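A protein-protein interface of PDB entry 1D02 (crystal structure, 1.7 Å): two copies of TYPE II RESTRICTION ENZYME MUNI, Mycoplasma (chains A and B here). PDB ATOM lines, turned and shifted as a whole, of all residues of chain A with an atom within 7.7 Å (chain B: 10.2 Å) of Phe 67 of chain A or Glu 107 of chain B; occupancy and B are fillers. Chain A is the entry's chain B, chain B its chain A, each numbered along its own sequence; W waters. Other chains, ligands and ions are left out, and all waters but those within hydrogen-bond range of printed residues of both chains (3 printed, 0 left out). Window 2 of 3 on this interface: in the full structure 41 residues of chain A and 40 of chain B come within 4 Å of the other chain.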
ATOM      1  N   LEU A  58      21.682   2.281  13.868  1.00  0.00           N
ATOM      2  CA  LEU A  58      20.545   1.553  14.428  1.00  0.00           C
ATOM      3  C   LEU A  58      20.113   0.519  13.388  1.00  0.00           C
ATOM      4  O   LEU A  58      20.065   0.817  12.192  1.00  0.00           O
ATOM      5  CB  LEU A  58      19.358   2.496  14.693  1.00  0.00           C
ATOM      6  CG  LEU A  58      19.579   3.610  15.724  1.00  0.00           C
ATOM      7  CD1 LEU A  58      18.275   4.409  15.870  1.00  0.00           C
ATOM      8  CD2 LEU A  58      19.985   3.020  17.075  1.00  0.00           C
ATOM      9  N   VAL A  62      14.932  -1.379  14.146  1.00  0.00           N
ATOM     10  CA  VAL A  62      14.743  -0.390  15.193  1.00  0.00           C
ATOM     11  C   VAL A  62      14.292   0.888  14.483  1.00  0.00           C
ATOM     12  O   VAL A  62      13.361   1.570  14.924  1.00  0.00           O
ATOM     13  CB  VAL A  62      16.040  -0.115  16.002  1.00  0.00           C
ATOM     14  CG1 VAL A  62      15.896   1.188  16.809  1.00  0.00           C
ATOM     15  CG2 VAL A  62      16.293  -1.288  16.976  1.00  0.00           C
ATOM     16  N   ILE A  63      14.937   1.203  13.362  1.00  0.00           N
ATOM     17  CA  ILE A  63      14.549   2.380  12.591  1.00  0.00           C
ATOM     18  C   ILE A  63      13.053   2.338  12.316  1.00  0.00           C
ATOM     19  O   ILE A  63      12.353   3.340  12.445  1.00  0.00           O
ATOM     20  CB  ILE A  63      15.303   2.412  11.235  1.00  0.00           C
ATOM     21  CG1 ILE A  63      16.796   2.605  11.489  1.00  0.00           C
ATOM     22  CG2 ILE A  63      14.759   3.511  10.351  1.00  0.00           C
ATOM     23  CD1 ILE A  63      17.149   3.981  12.029  1.00  0.00           C
ATOM     24  N   LYS A  64      12.560   1.167  11.930  1.00  0.00           N
ATOM     25  CA  LYS A  64      11.145   1.029  11.627  1.00  0.00           C
ATOM     26  C   LYS A  64      10.217   1.363  12.799  1.00  0.00           C
ATOM     27  O   LYS A  64       9.078   1.782  12.579  1.00  0.00           O
ATOM     28  CB  LYS A  64      10.859  -0.393  11.124  1.00  0.00           C
ATOM     29  CG  LYS A  64       9.416  -0.610  10.701  1.00  0.00           C
ATOM     30  CD  LYS A  64       9.225  -1.912   9.930  1.00  0.00           C
ATOM     31  CE  LYS A  64       7.789  -2.018   9.406  1.00  0.00           C
ATOM     32  NZ  LYS A  64       7.605  -3.187   8.498  1.00  0.00           N
ATOM     33  N   GLU A  65      10.703   1.217  14.029  1.00  0.00           N
ATOM     34  CA  GLU A  65       9.861   1.471  15.195  1.00  0.00           C
ATOM     35  C   GLU A  65      10.013   2.837  15.861  1.00  0.00           C
ATOM     36  O   GLU A  65       9.304   3.129  16.836  1.00  0.00           O
ATOM     37  CB  GLU A  65      10.106   0.392  16.252  1.00  0.00           C
ATOM     38  CG  GLU A  65       9.978  -1.046  15.754  1.00  0.00           C
ATOM     39  CD  GLU A  65       8.640  -1.340  15.102  1.00  0.00           C
ATOM     40  OE1 GLU A  65       7.604  -0.834  15.592  1.00  0.00           O
ATOM     41  OE2 GLU A  65       8.619  -2.089  14.100  1.00  0.00           O
ATOM     42  N   ILE A  66      10.914   3.685  15.371  1.00  0.00           N
ATOM     43  CA  ILE A  66      11.095   4.975  16.022  1.00  0.00           C
ATOM     44  C   ILE A  66      10.668   6.128  15.134  1.00  0.00           C
ATOM     45  O   ILE A  66      10.264   5.923  13.985  1.00  0.00           O
ATOM     46  CB  ILE A  66      12.576   5.229  16.423  1.00  0.00           C
ATOM     47  CG1 ILE A  66      13.461   5.384  15.185  1.00  0.00           C
ATOM     48  CG2 ILE A  66      13.082   4.085  17.280  1.00  0.00           C
ATOM     49  CD1 ILE A  66      14.859   5.959  15.505  1.00  0.00           C
ATOM     50  N   PHE A  67      10.732   7.336  15.683  1.00  0.00           N
ATOM     51  CA  PHE A  67      10.403   8.536  14.914  1.00  0.00           C
ATOM     52  C   PHE A  67      11.685   8.916  14.180  1.00  0.00           C
ATOM     53  O   PHE A  67      12.739   9.055  14.808  1.00  0.00           O
ATOM     54  CB  PHE A  67       9.983   9.675  15.844  1.00  0.00           C
ATOM     55  CG  PHE A  67       9.979  11.025  15.179  1.00  0.00           C
ATOM     56  CD1 PHE A  67       9.276  11.221  13.987  1.00  0.00           C
ATOM     57  CD2 PHE A  67      10.649  12.108  15.750  1.00  0.00           C
ATOM     58  CE1 PHE A  67       9.240  12.483  13.384  1.00  0.00           C
ATOM     59  CE2 PHE A  67      10.618  13.374  15.154  1.00  0.00           C
ATOM     60  CZ  PHE A  67       9.907  13.560  13.963  1.00  0.00           C
ATOM     61  N   ASN A  68      11.596   9.081  12.860  1.00  0.00           N
ATOM     62  CA  ASN A  68      12.753   9.439  12.048  1.00  0.00           C
ATOM     63  C   ASN A  68      12.540  10.810  11.406  1.00  0.00           C
ATOM     64  O   ASN A  68      11.966  10.922  10.334  1.00  0.00           O
ATOM     65  CB  ASN A  68      12.973   8.368  10.981  1.00  0.00           C
ATOM     66  CG  ASN A  68      13.345   7.023  11.587  1.00  0.00           C
ATOM     67  OD1 ASN A  68      14.462   6.841  12.092  1.00  0.00           O
ATOM     68  ND2 ASN A  68      12.408   6.085  11.556  1.00  0.00           N
ATOM     69  N   PRO A  69      13.011  11.874  12.065  1.00  0.00           N
ATOM     70  CA  PRO A  69      12.837  13.214  11.512  1.00  0.00           C
ATOM     71  C   PRO A  69      13.491  13.410  10.158  1.00  0.00           C
ATOM     72  O   PRO A  69      14.510  12.788   9.823  1.00  0.00           O
ATOM     73  CB  PRO A  69      13.419  14.118  12.592  1.00  0.00           C
ATOM     74  CG  PRO A  69      14.463  13.216  13.263  1.00  0.00           C
ATOM     75  CD  PRO A  69      13.723  11.911  13.353  1.00  0.00           C
ATOM     76  N   LEU A  70      12.874  14.286   9.375  1.00  0.00           N
ATOM     77  CA  LEU A  70      13.359  14.580   8.040  1.00  0.00           C
ATOM     78  C   LEU A  70      14.520  15.570   8.061  1.00  0.00           C
ATOM     79  O   LEU A  70      14.403  16.713   7.572  1.00  0.00           O
ATOM     80  CB  LEU A  70      12.192  15.133   7.211  1.00  0.00           C
ATOM     81  CG  LEU A  70      11.072  14.107   6.999  1.00  0.00           C
ATOM     82  CD1 LEU A  70       9.775  14.817   6.588  1.00  0.00           C
ATOM     83  CD2 LEU A  70      11.509  13.062   5.928  1.00  0.00           C
ATOM     84  N   LEU A  73      21.054  13.445   9.316  1.00  0.00           N
ATOM     85  CA  LEU A  73      21.800  13.033  10.499  1.00  0.00           C
ATOM     86  C   LEU A  73      23.301  13.055  10.260  1.00  0.00           C
ATOM     87  O   LEU A  73      24.077  13.208  11.210  1.00  0.00           O
ATOM     88  CB  LEU A  73      21.356  11.627  10.962  1.00  0.00           C
ATOM     89  CG  LEU A  73      19.899  11.602  11.472  1.00  0.00           C
ATOM     90  CD1 LEU A  73      19.501  10.180  11.867  1.00  0.00           C
ATOM     91  CD2 LEU A  73      19.759  12.561  12.666  1.00  0.00           C
ATOM     92  N   TRP A  78      24.702  16.101  17.834  1.00  0.00           N
ATOM     93  CA  TRP A  78      24.048  15.830  19.118  1.00  0.00           C
ATOM     94  C   TRP A  78      25.119  15.275  20.047  1.00  0.00           C
ATOM     95  O   TRP A  78      25.788  14.284  19.739  1.00  0.00           O
ATOM     96  CB  TRP A  78      22.916  14.797  18.990  1.00  0.00           C
ATOM     97  CG  TRP A  78      21.749  15.254  18.168  1.00  0.00           C
ATOM     98  CD1 TRP A  78      21.339  16.546  17.958  1.00  0.00           C
ATOM     99  CD2 TRP A  78      20.815  14.418  17.496  1.00  0.00           C
ATOM    100  NE1 TRP A  78      20.186  16.560  17.193  1.00  0.00           N
ATOM    101  CE2 TRP A  78      19.847  15.264  16.896  1.00  0.00           C
ATOM    102  CE3 TRP A  78      20.695  13.026  17.341  1.00  0.00           C
ATOM    103  CZ2 TRP A  78      18.774  14.765  16.160  1.00  0.00           C
ATOM    104  CZ3 TRP A  78      19.624  12.532  16.606  1.00  0.00           C
ATOM    105  CH2 TRP A  78      18.676  13.405  16.024  1.00  0.00           C
ATOM    106  N   GLY B 104       9.410  12.178  25.041  1.00  0.00           N
ATOM    107  CA  GLY B 104      10.426  12.254  24.005  1.00  0.00           C
ATOM    108  C   GLY B 104       9.979  13.022  22.776  1.00  0.00           C
ATOM    109  O   GLY B 104       8.797  13.381  22.637  1.00  0.00           O
ATOM    110  N   TRP B 105      10.944  13.285  21.900  1.00  0.00           N
ATOM    111  CA  TRP B 105      10.682  13.987  20.660  1.00  0.00           C
ATOM    112  C   TRP B 105      10.211  12.936  19.671  1.00  0.00           C
ATOM    113  O   TRP B 105      10.982  12.042  19.269  1.00  0.00           O
ATOM    114  CB  TRP B 105      11.972  14.685  20.219  1.00  0.00           C
ATOM    115  CG  TRP B 105      12.018  15.250  18.832  1.00  0.00           C
ATOM    116  CD1 TRP B 105      10.997  15.804  18.120  1.00  0.00           C
ATOM    117  CD2 TRP B 105      13.198  15.368  18.017  1.00  0.00           C
ATOM    118  NE1 TRP B 105      11.477  16.278  16.902  1.00  0.00           N
ATOM    119  CE2 TRP B 105      12.819  16.016  16.821  1.00  0.00           C
ATOM    120  CE3 TRP B 105      14.536  14.987  18.193  1.00  0.00           C
ATOM    121  CZ2 TRP B 105      13.735  16.292  15.801  1.00  0.00           C
ATOM    122  CZ3 TRP B 105      15.450  15.260  17.179  1.00  0.00           C
ATOM    123  CH2 TRP B 105      15.042  15.905  16.000  1.00  0.00           C
ATOM    124  N   VAL B 106       8.924  13.013  19.319  1.00  0.00           N
ATOM    125  CA  VAL B 106       8.326  12.083  18.376  1.00  0.00           C
ATOM    126  C   VAL B 106       7.456  12.850  17.370  1.00  0.00           C
ATOM    127  O   VAL B 106       7.371  14.073  17.429  1.00  0.00           O
ATOM    128  CB  VAL B 106       7.483  10.993  19.099  1.00  0.00           C
ATOM    129  CG1 VAL B 106       8.391  10.136  20.016  1.00  0.00           C
ATOM    130  CG2 VAL B 106       6.359  11.643  19.897  1.00  0.00           C
ATOM    131  N   GLU B 107       6.793  12.146  16.458  1.00  0.00           N
ATOM    132  CA  GLU B 107       6.019  12.886  15.464  1.00  0.00           C
ATOM    133  C   GLU B 107       5.017  13.864  16.064  1.00  0.00           C
ATOM    134  O   GLU B 107       4.363  13.594  17.080  1.00  0.00           O
ATOM    135  CB  GLU B 107       5.348  11.963  14.417  1.00  0.00           C
ATOM    136  CG  GLU B 107       4.883  10.566  14.793  1.00  0.00           C
ATOM    137  CD  GLU B 107       6.023   9.586  15.106  1.00  0.00           C
ATOM    138  OE1 GLU B 107       6.407   9.542  16.269  1.00  0.00           O
ATOM    139  OE2 GLU B 107       6.528   8.873  14.204  1.00  0.00           O
ATOM    140  N   GLY B 108       4.960  15.048  15.458  1.00  0.00           N
ATOM    141  CA  GLY B 108       4.054  16.077  15.929  1.00  0.00           C
ATOM    142  C   GLY B 108       4.603  16.917  17.070  1.00  0.00           C
ATOM    143  O   GLY B 108       3.932  17.857  17.515  1.00  0.00           O
ATOM    144  N   LYS B 109       5.812  16.605  17.551  1.00  0.00           N
ATOM    145  CA  LYS B 109       6.396  17.360  18.654  1.00  0.00           C
ATOM    146  C   LYS B 109       7.721  17.969  18.250  1.00  0.00           C
ATOM    147  O   LYS B 109       8.333  17.550  17.270  1.00  0.00           O
ATOM    148  CB  LYS B 109       6.585  16.453  19.879  1.00  0.00           C
ATOM    149  CG  LYS B 109       5.303  15.692  20.258  1.00  0.00           C
ATOM    150  CD  LYS B 109       5.449  14.984  21.579  1.00  0.00           C
ATOM    151  CE  LYS B 109       4.201  14.178  21.937  1.00  0.00           C
ATOM    152  NZ  LYS B 109       3.045  15.077  22.127  1.00  0.00           N
ATOM    153  N   ASP B 110       8.133  18.995  18.986  1.00  0.00           N
ATOM    154  CA  ASP B 110       9.396  19.664  18.728  1.00  0.00           C
ATOM    155  C   ASP B 110      10.467  18.942  19.532  1.00  0.00           C
ATOM    156  O   ASP B 110      10.151  18.204  20.474  1.00  0.00           O
ATOM    157  CB  ASP B 110       9.338  21.115  19.195  1.00  0.00           C
ATOM    158  CG  ASP B 110       8.784  22.050  18.138  1.00  0.00           C
ATOM    159  OD1 ASP B 110       8.271  21.571  17.104  1.00  0.00           O
ATOM    160  OD2 ASP B 110       8.875  23.274  18.354  1.00  0.00           O
ATOM    161  N   PRO B 111      11.742  19.140  19.172  1.00  0.00           N
ATOM    162  CA  PRO B 111      12.849  18.497  19.884  1.00  0.00           C
ATOM    163  C   PRO B 111      12.810  18.782  21.387  1.00  0.00           C
ATOM    164  O   PRO B 111      13.260  17.966  22.187  1.00  0.00           O
ATOM    165  CB  PRO B 111      14.076  19.116  19.233  1.00  0.00           C
ATOM    166  CG  PRO B 111      13.615  19.322  17.797  1.00  0.00           C
ATOM    167  CD  PRO B 111      12.236  19.883  17.991  1.00  0.00           C
ATOM    168  N   SER B 112      12.273  19.937  21.772  1.00  0.00           N
ATOM    169  CA  SER B 112      12.198  20.292  23.187  1.00  0.00           C
ATOM    170  C   SER B 112      11.371  19.279  23.992  1.00  0.00           C
ATOM    171  O   SER B 112      11.567  19.138  25.202  1.00  0.00           O
ATOM    172  CB  SER B 112      11.611  21.704  23.351  1.00  0.00           C
ATOM    173  OG  SER B 112      10.277  21.785  22.827  1.00  0.00           O
ATOM    174  N   ALA B 113      10.456  18.553  23.343  1.00  0.00           N
ATOM    175  CA  ALA B 113       9.666  17.580  24.086  1.00  0.00           C
ATOM    176  C   ALA B 113      10.581  16.457  24.559  1.00  0.00           C
ATOM    177  O   ALA B 113      10.251  15.745  25.504  1.00  0.00           O
ATOM    178  CB  ALA B 113       8.524  17.008  23.242  1.00  0.00           C
ATOM    179  N   GLY B 114      11.750  16.327  23.938  1.00  0.00           N
ATOM    180  CA  GLY B 114      12.654  15.280  24.376  1.00  0.00           C
ATOM    181  C   GLY B 114      13.860  15.836  25.110  1.00  0.00           C
ATOM    182  O   GLY B 114      14.866  15.146  25.233  1.00  0.00           O
ATOM    183  N   GLY B 154       7.735   4.836  27.421  1.00  0.00           N
ATOM    184  CA  GLY B 154       7.320   6.182  27.061  1.00  0.00           C
ATOM    185  C   GLY B 154       7.866   6.636  25.714  1.00  0.00           C
ATOM    186  O   GLY B 154       8.575   5.886  25.030  1.00  0.00           O
ATOM    187  N   ASP B 155       7.575   7.874  25.341  1.00  0.00           N
ATOM    188  CA  ASP B 155       8.030   8.372  24.048  1.00  0.00           C
ATOM    189  C   ASP B 155       9.557   8.424  23.912  1.00  0.00           C
ATOM    190  O   ASP B 155      10.066   8.459  22.794  1.00  0.00           O
ATOM    191  CB  ASP B 155       7.429   9.741  23.770  1.00  0.00           C
ATOM    192  CG  ASP B 155       5.954   9.661  23.382  1.00  0.00           C
ATOM    193  OD1 ASP B 155       5.263  10.694  23.497  1.00  0.00           O
ATOM    194  OD2 ASP B 155       5.507   8.572  22.962  1.00  0.00           O
ATOM    195  N   ILE B 156      10.281   8.418  25.029  1.00  0.00           N
ATOM    196  CA  ILE B 156      11.746   8.414  24.941  1.00  0.00           C
ATOM    197  C   ILE B 156      12.191   7.215  24.088  1.00  0.00           C
ATOM    198  O   ILE B 156      13.191   7.285  23.372  1.00  0.00           O
ATOM    199  CB  ILE B 156      12.402   8.296  26.349  1.00  0.00           C
ATOM    200  CG1 ILE B 156      13.932   8.401  26.234  1.00  0.00           C
ATOM    201  CG2 ILE B 156      12.015   6.974  27.011  1.00  0.00           C
ATOM    202  CD1 ILE B 156      14.626   8.451  27.622  1.00  0.00           C
ATOM    203  N   THR B 157      11.421   6.129  24.123  1.00  0.00           N
ATOM    204  CA  THR B 157      11.800   4.943  23.371  1.00  0.00           C
ATOM    205  C   THR B 157      11.678   5.085  21.851  1.00  0.00           C
ATOM    206  O   THR B 157      12.099   4.191  21.118  1.00  0.00           O
ATOM    207  CB  THR B 157      10.959   3.703  23.766  1.00  0.00           C
ATOM    208  OG1 THR B 157       9.590   3.947  23.429  1.00  0.00           O
ATOM    209  CG2 THR B 157      11.052   3.424  25.273  1.00  0.00           C
ATOM    210  N   ARG B 158      11.097   6.177  21.376  1.00  0.00           N
ATOM    211  CA  ARG B 158      10.968   6.371  19.922  1.00  0.00           C
ATOM    212  C   ARG B 158      11.637   7.664  19.488  1.00  0.00           C
ATOM    213  O   ARG B 158      11.544   8.074  18.336  1.00  0.00           O
ATOM    214  CB  ARG B 158       9.490   6.392  19.499  1.00  0.00           C
ATOM    215  CG  ARG B 158       8.771   5.059  19.752  1.00  0.00           C
ATOM    216  CD  ARG B 158       7.357   5.038  19.117  1.00  0.00           C
ATOM    217  NE  ARG B 158       7.440   5.164  17.673  1.00  0.00           N
ATOM    218  CZ  ARG B 158       7.163   6.271  16.994  1.00  0.00           C
ATOM    219  NH1 ARG B 158       6.760   7.376  17.627  1.00  0.00           N
ATOM    220  NH2 ARG B 158       7.316   6.287  15.677  1.00  0.00           N
ATOM    221  N   ASP B 159      12.319   8.299  20.432  1.00  0.00           N
ATOM    222  CA  ASP B 159      13.000   9.568  20.207  1.00  0.00           C
ATOM    223  C   ASP B 159      14.319   9.254  19.465  1.00  0.00           C
ATOM    224  O   ASP B 159      15.143   8.474  19.960  1.00  0.00           O
ATOM    225  CB  ASP B 159      13.221  10.197  21.589  1.00  0.00           C
ATOM    226  CG  ASP B 159      13.943  11.524  21.540  1.00  0.00           C
ATOM    227  OD1 ASP B 159      14.964  11.615  20.815  1.00  0.00           O
ATOM    228  OD2 ASP B 159      13.492  12.465  22.258  1.00  0.00           O
ATOM    229  N   PRO B 160      14.541   9.857  18.280  1.00  0.00           N
ATOM    230  CA  PRO B 160      15.761   9.589  17.492  1.00  0.00           C
ATOM    231  C   PRO B 160      17.070   9.933  18.171  1.00  0.00           C
ATOM    232  O   PRO B 160      18.107   9.311  17.907  1.00  0.00           O
ATOM    233  CB  PRO B 160      15.547  10.421  16.223  1.00  0.00           C
ATOM    234  CG  PRO B 160      14.724  11.588  16.732  1.00  0.00           C
ATOM    235  CD  PRO B 160      13.712  10.884  17.614  1.00  0.00           C
ATOM    236  N   LYS B 161      17.010  10.937  19.041  1.00  0.00           N
ATOM    237  CA  LYS B 161      18.192  11.399  19.758  1.00  0.00           C
ATOM    238  C   LYS B 161      18.420  10.541  21.000  1.00  0.00           C
ATOM    239  O   LYS B 161      19.519  10.037  21.223  1.00  0.00           O
ATOM    240  CB  LYS B 161      18.021  12.874  20.163  1.00  0.00           C
ATOM    241  CG  LYS B 161      19.230  13.457  20.901  1.00  0.00           C
ATOM    242  CD  LYS B 161      19.013  14.912  21.355  1.00  0.00           C
ATOM    243  CE  LYS B 161      18.629  15.841  20.209  1.00  0.00           C
ATOM    244  NZ  LYS B 161      18.550  17.298  20.669  1.00  0.00           N
ATOM    245  N   ARG B 162      17.371  10.350  21.800  1.00  0.00           N
ATOM    246  CA  ARG B 162      17.505   9.535  23.017  1.00  0.00           C
ATOM    247  C   ARG B 162      17.854   8.081  22.717  1.00  0.00           C
ATOM    248  O   ARG B 162      18.644   7.464  23.426  1.00  0.00           O
ATOM    249  CB  ARG B 162      16.203   9.569  23.834  1.00  0.00           C
ATOM    250  CG  ARG B 162      15.879  10.945  24.419  1.00  0.00           C
ATOM    251  CD  ARG B 162      16.609  11.218  25.752  1.00  0.00           C
ATOM    252  NE  ARG B 162      16.686  12.669  25.958  1.00  0.00           N
ATOM    253  CZ  ARG B 162      17.756  13.407  25.678  1.00  0.00           C
ATOM    254  NH1 ARG B 162      18.862  12.828  25.218  1.00  0.00           N
ATOM    255  NH2 ARG B 162      17.689  14.732  25.783  1.00  0.00           N
ATOM    256  N   VAL B 163      17.252   7.520  21.673  1.00  0.00           N
ATOM    257  CA  VAL B 163      17.543   6.139  21.353  1.00  0.00           C
ATOM    258  C   VAL B 163      19.015   5.989  20.962  1.00  0.00           C
ATOM    259  O   VAL B 163      19.691   5.069  21.408  1.00  0.00           O
ATOM    260  CB  VAL B 163      16.628   5.620  20.229  1.00  0.00           C
ATOM    261  CG1 VAL B 163      17.128   4.286  19.709  1.00  0.00           C
ATOM    262  CG2 VAL B 163      15.213   5.416  20.781  1.00  0.00           C
ATOM    263  N   ARG B 164      19.520   6.908  20.158  1.00  0.00           N
ATOM    264  CA  ARG B 164      20.926   6.816  19.767  1.00  0.00           C
ATOM    265  C   ARG B 164      21.858   7.112  20.939  1.00  0.00           C
ATOM    266  O   ARG B 164      22.909   6.494  21.066  1.00  0.00           O
ATOM    267  CB  ARG B 164      21.208   7.758  18.600  1.00  0.00           C
ATOM    268  CG  ARG B 164      20.575   7.243  17.310  1.00  0.00           C
ATOM    269  CD  ARG B 164      20.895   8.142  16.135  1.00  0.00           C
ATOM    270  NE  ARG B 164      20.384   7.580  14.884  1.00  0.00           N
ATOM    271  CZ  ARG B 164      19.141   7.721  14.434  1.00  0.00           C
ATOM    272  NH1 ARG B 164      18.243   8.424  15.125  1.00  0.00           N
ATOM    273  NH2 ARG B 164      18.797   7.135  13.287  1.00  0.00           N
ATOM    274  N   ARG B 181       8.399  -0.118  23.655  1.00  0.00           N
ATOM    275  CA  ARG B 181       7.703   0.948  22.957  1.00  0.00           C
ATOM    276  C   ARG B 181       6.196   0.995  23.127  1.00  0.00           C
ATOM    277  O   ARG B 181       5.546  -0.014  23.439  1.00  0.00           O
ATOM    278  CB  ARG B 181       8.106   0.917  21.468  1.00  0.00           C
ATOM    279  CG  ARG B 181       9.619   1.116  21.275  1.00  0.00           C
ATOM    280  CD  ARG B 181      10.101   1.228  19.816  1.00  0.00           C
ATOM    281  NE  ARG B 181      11.446   1.815  19.865  1.00  0.00           N
ATOM    282  CZ  ARG B 181      12.598   1.145  19.823  1.00  0.00           C
ATOM    283  NH1 ARG B 181      12.627  -0.183  19.687  1.00  0.00           N
ATOM    284  NH2 ARG B 181      13.731   1.813  19.976  1.00  0.00           N
ATOM    285  N   PRO B 182       5.612   2.179  22.927  1.00  0.00           N
ATOM    286  CA  PRO B 182       4.160   2.331  23.080  1.00  0.00           C
ATOM    287  C   PRO B 182       3.367   1.289  22.296  1.00  0.00           C
ATOM    288  O   PRO B 182       3.711   0.946  21.163  1.00  0.00           O
ATOM    289  CB  PRO B 182       3.913   3.757  22.591  1.00  0.00           C
ATOM    290  CG  PRO B 182       5.214   4.464  22.997  1.00  0.00           C
ATOM    291  CD  PRO B 182       6.242   3.462  22.557  1.00  0.00           C
ATOM    292  N   ASN B 183       2.331   0.759  22.935  1.00  0.00           N
ATOM    293  CA  ASN B 183       1.475  -0.242  22.303  1.00  0.00           C
ATOM    294  C   ASN B 183       2.114  -1.600  22.070  1.00  0.00           C
ATOM    295  O   ASN B 183       1.508  -2.464  21.433  1.00  0.00           O
ATOM    296  CB  ASN B 183       0.937   0.299  20.979  1.00  0.00           C
ATOM    297  CG  ASN B 183       0.288   1.653  21.143  1.00  0.00           C
ATOM    298  OD1 ASN B 183      -0.453   1.878  22.103  1.00  0.00           O
ATOM    299  ND2 ASN B 183       0.566   2.567  20.218  1.00  0.00           N
HETATM  300  O   HOH W   1       7.690   4.077  13.701  1.00  0.00           O
HETATM  301  O   HOH W   2       6.891   1.776  17.747  1.00  0.00           O
HETATM  302  O   HOH W   3      16.182   8.725  13.050  1.00  0.00           O
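NE of Arg 158 of chain B lies within hydrogen-bond range of O of Glu 65 of chain A (2.9 Å). The backbone carbonyl oxygen (O) of Arg 158 of chain B sits at hydrogen-bond distance from the backbone NH (N) of Phe 67 of chain A. NH2 of Arg 158 of chain B lies close to O of Ile 66 of chain A (3.4 Å).
The side-chain carboxylate of Asp 159 of chain B sits at hydrogen-bond distance from the backbone NH of Lys 161 of chain B (2.8 Å). The backbone carbonyl oxygen (O) of Ile 66 of chain A lies within hydrogen-bond range of the side-chain amide nitrogen (ND2) of Asn 68 of chain A, at 3.2 Å. The side-chain hydroxyl (OG1) of Thr 157 of chain B sits at hydrogen-bond distance from the backbone carbonyl oxygen (O) of Gly 154 of chain B (2.7 Å). NH1 of Arg 158 of chain B lies within salt-bridge range of OE1 of Glu 107 of chain B (2.6 Å). O of Thr 157 of chain B is in hydrogen-bond range of NE of Arg 181 of chain B (2.8 Å). O of Pro 160 of chain B is in hydrogen-bond range of NH1 of Arg 164 of chain B (2.9 Å).
Among the printed residues, pairs that only touch across the chains: Leu 58 of chain A with Arg 164 of chain B (3.7 Å), Val 62 of chain A with Arg 181 of chain B (3.9 Å), Ile 63 of chain A with Arg 164 of chain B (3.8 Å), Glu 65 of chain A with Arg 181 of chain B (3.6 Å), Ile 66 of chain A with Thr 157 of chain B (3.96 Å), Ile 66 of chain A with Arg 181 of chain B (3.6 Å), Phe 67 of chain A with Trp 105 of chain B (3.5 Å), Phe 67 of chain A with Val 106 of chain B (3.5 Å), Phe 67 of chain A with Glu 107 of chain B (3.6 Å), Phe 67 of chain A with Pro 160 of chain B (3.4 Å), Pro 69 of chain A with Trp 105 of chain B (3.9 Å), Pro 69 of chain A with Pro 160 of chain B (3.5 Å), Leu 73 of chain A with Arg 164 of chain B (3.4 Å), Trp 78 of chain A with Trp 105 of chain B (3.5 Å), Trp 78 of chain A with Pro 160 of chain B (3.8 Å) and Trp 78 of chain A with Lys 161 of chain B (3.5 Å).
Of the printed residues of chain B, Ile 66 of chain A touches Thr 157 (3.96 Å), Arg 158 (3.4 Å) and Arg 181 (3.6 Å). Printed residues of chain B within 4 Å of Phe 67 of chain A: Trp 105 (3.5 Å), Val 106 (3.5 Å), Glu 107 (3.6 Å), Arg 158 (2.9 Å) and Pro 160 (3.4 Å). Printed residues of chain A within 4 Å of Glu 107 of chain B: Phe 67. Of the printed residues of chain A, Arg 158 of chain B touches Glu 65, Ile 66 and Phe 67. Of the printed residues of chain A, Pro 160 of chain B touches Phe 67 (3.4 Å), Pro 69 (3.5 Å) and Trp 78 (3.8 Å). Printed residues of chain A within 4 Å of Lys 161 of chain B: Trp 78. The nearest printed residue of chain B that does not touch Trp 78 of chain A is Arg 164 of chain B (4.6 Å).
Of the 12 printed residues of chain A, 9 touch a printed residue of chain B. Of the 25 printed residues of chain B, 9 touch a printed residue of chain A. Printed residues of chain B that touch a printed residue of chain A: Trp 105, Val 106, Glu 107, Thr 157, Arg 158, Pro 160, Lys 161, Arg 164 and Arg 181. Hydrophobic or aromatic side chains of chain B that line the printed part of chain A: Trp 105 and Pro 160.
No position is printed for both chains.
Water W3 lies within hydrogen-bond range of OD1 of Asn 68 of chain A (2.7 Å) and NH1 of Arg 164 of chain B (2.9 Å). Water W1 lies within hydrogen-bond range of O of Lys 64 of chain A (2.9 Å), NH2 of Arg 158 of chain B (3.0 Å) and O of Ile 66 of chain A (3.2 Å). Water W2 lies within hydrogen-bond range of the backbone carbonyl oxygen (O) of Glu 65 of chain A (2.9 Å) and the guanidinium group (NE) of Arg 158 of chain B (3.4 Å).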
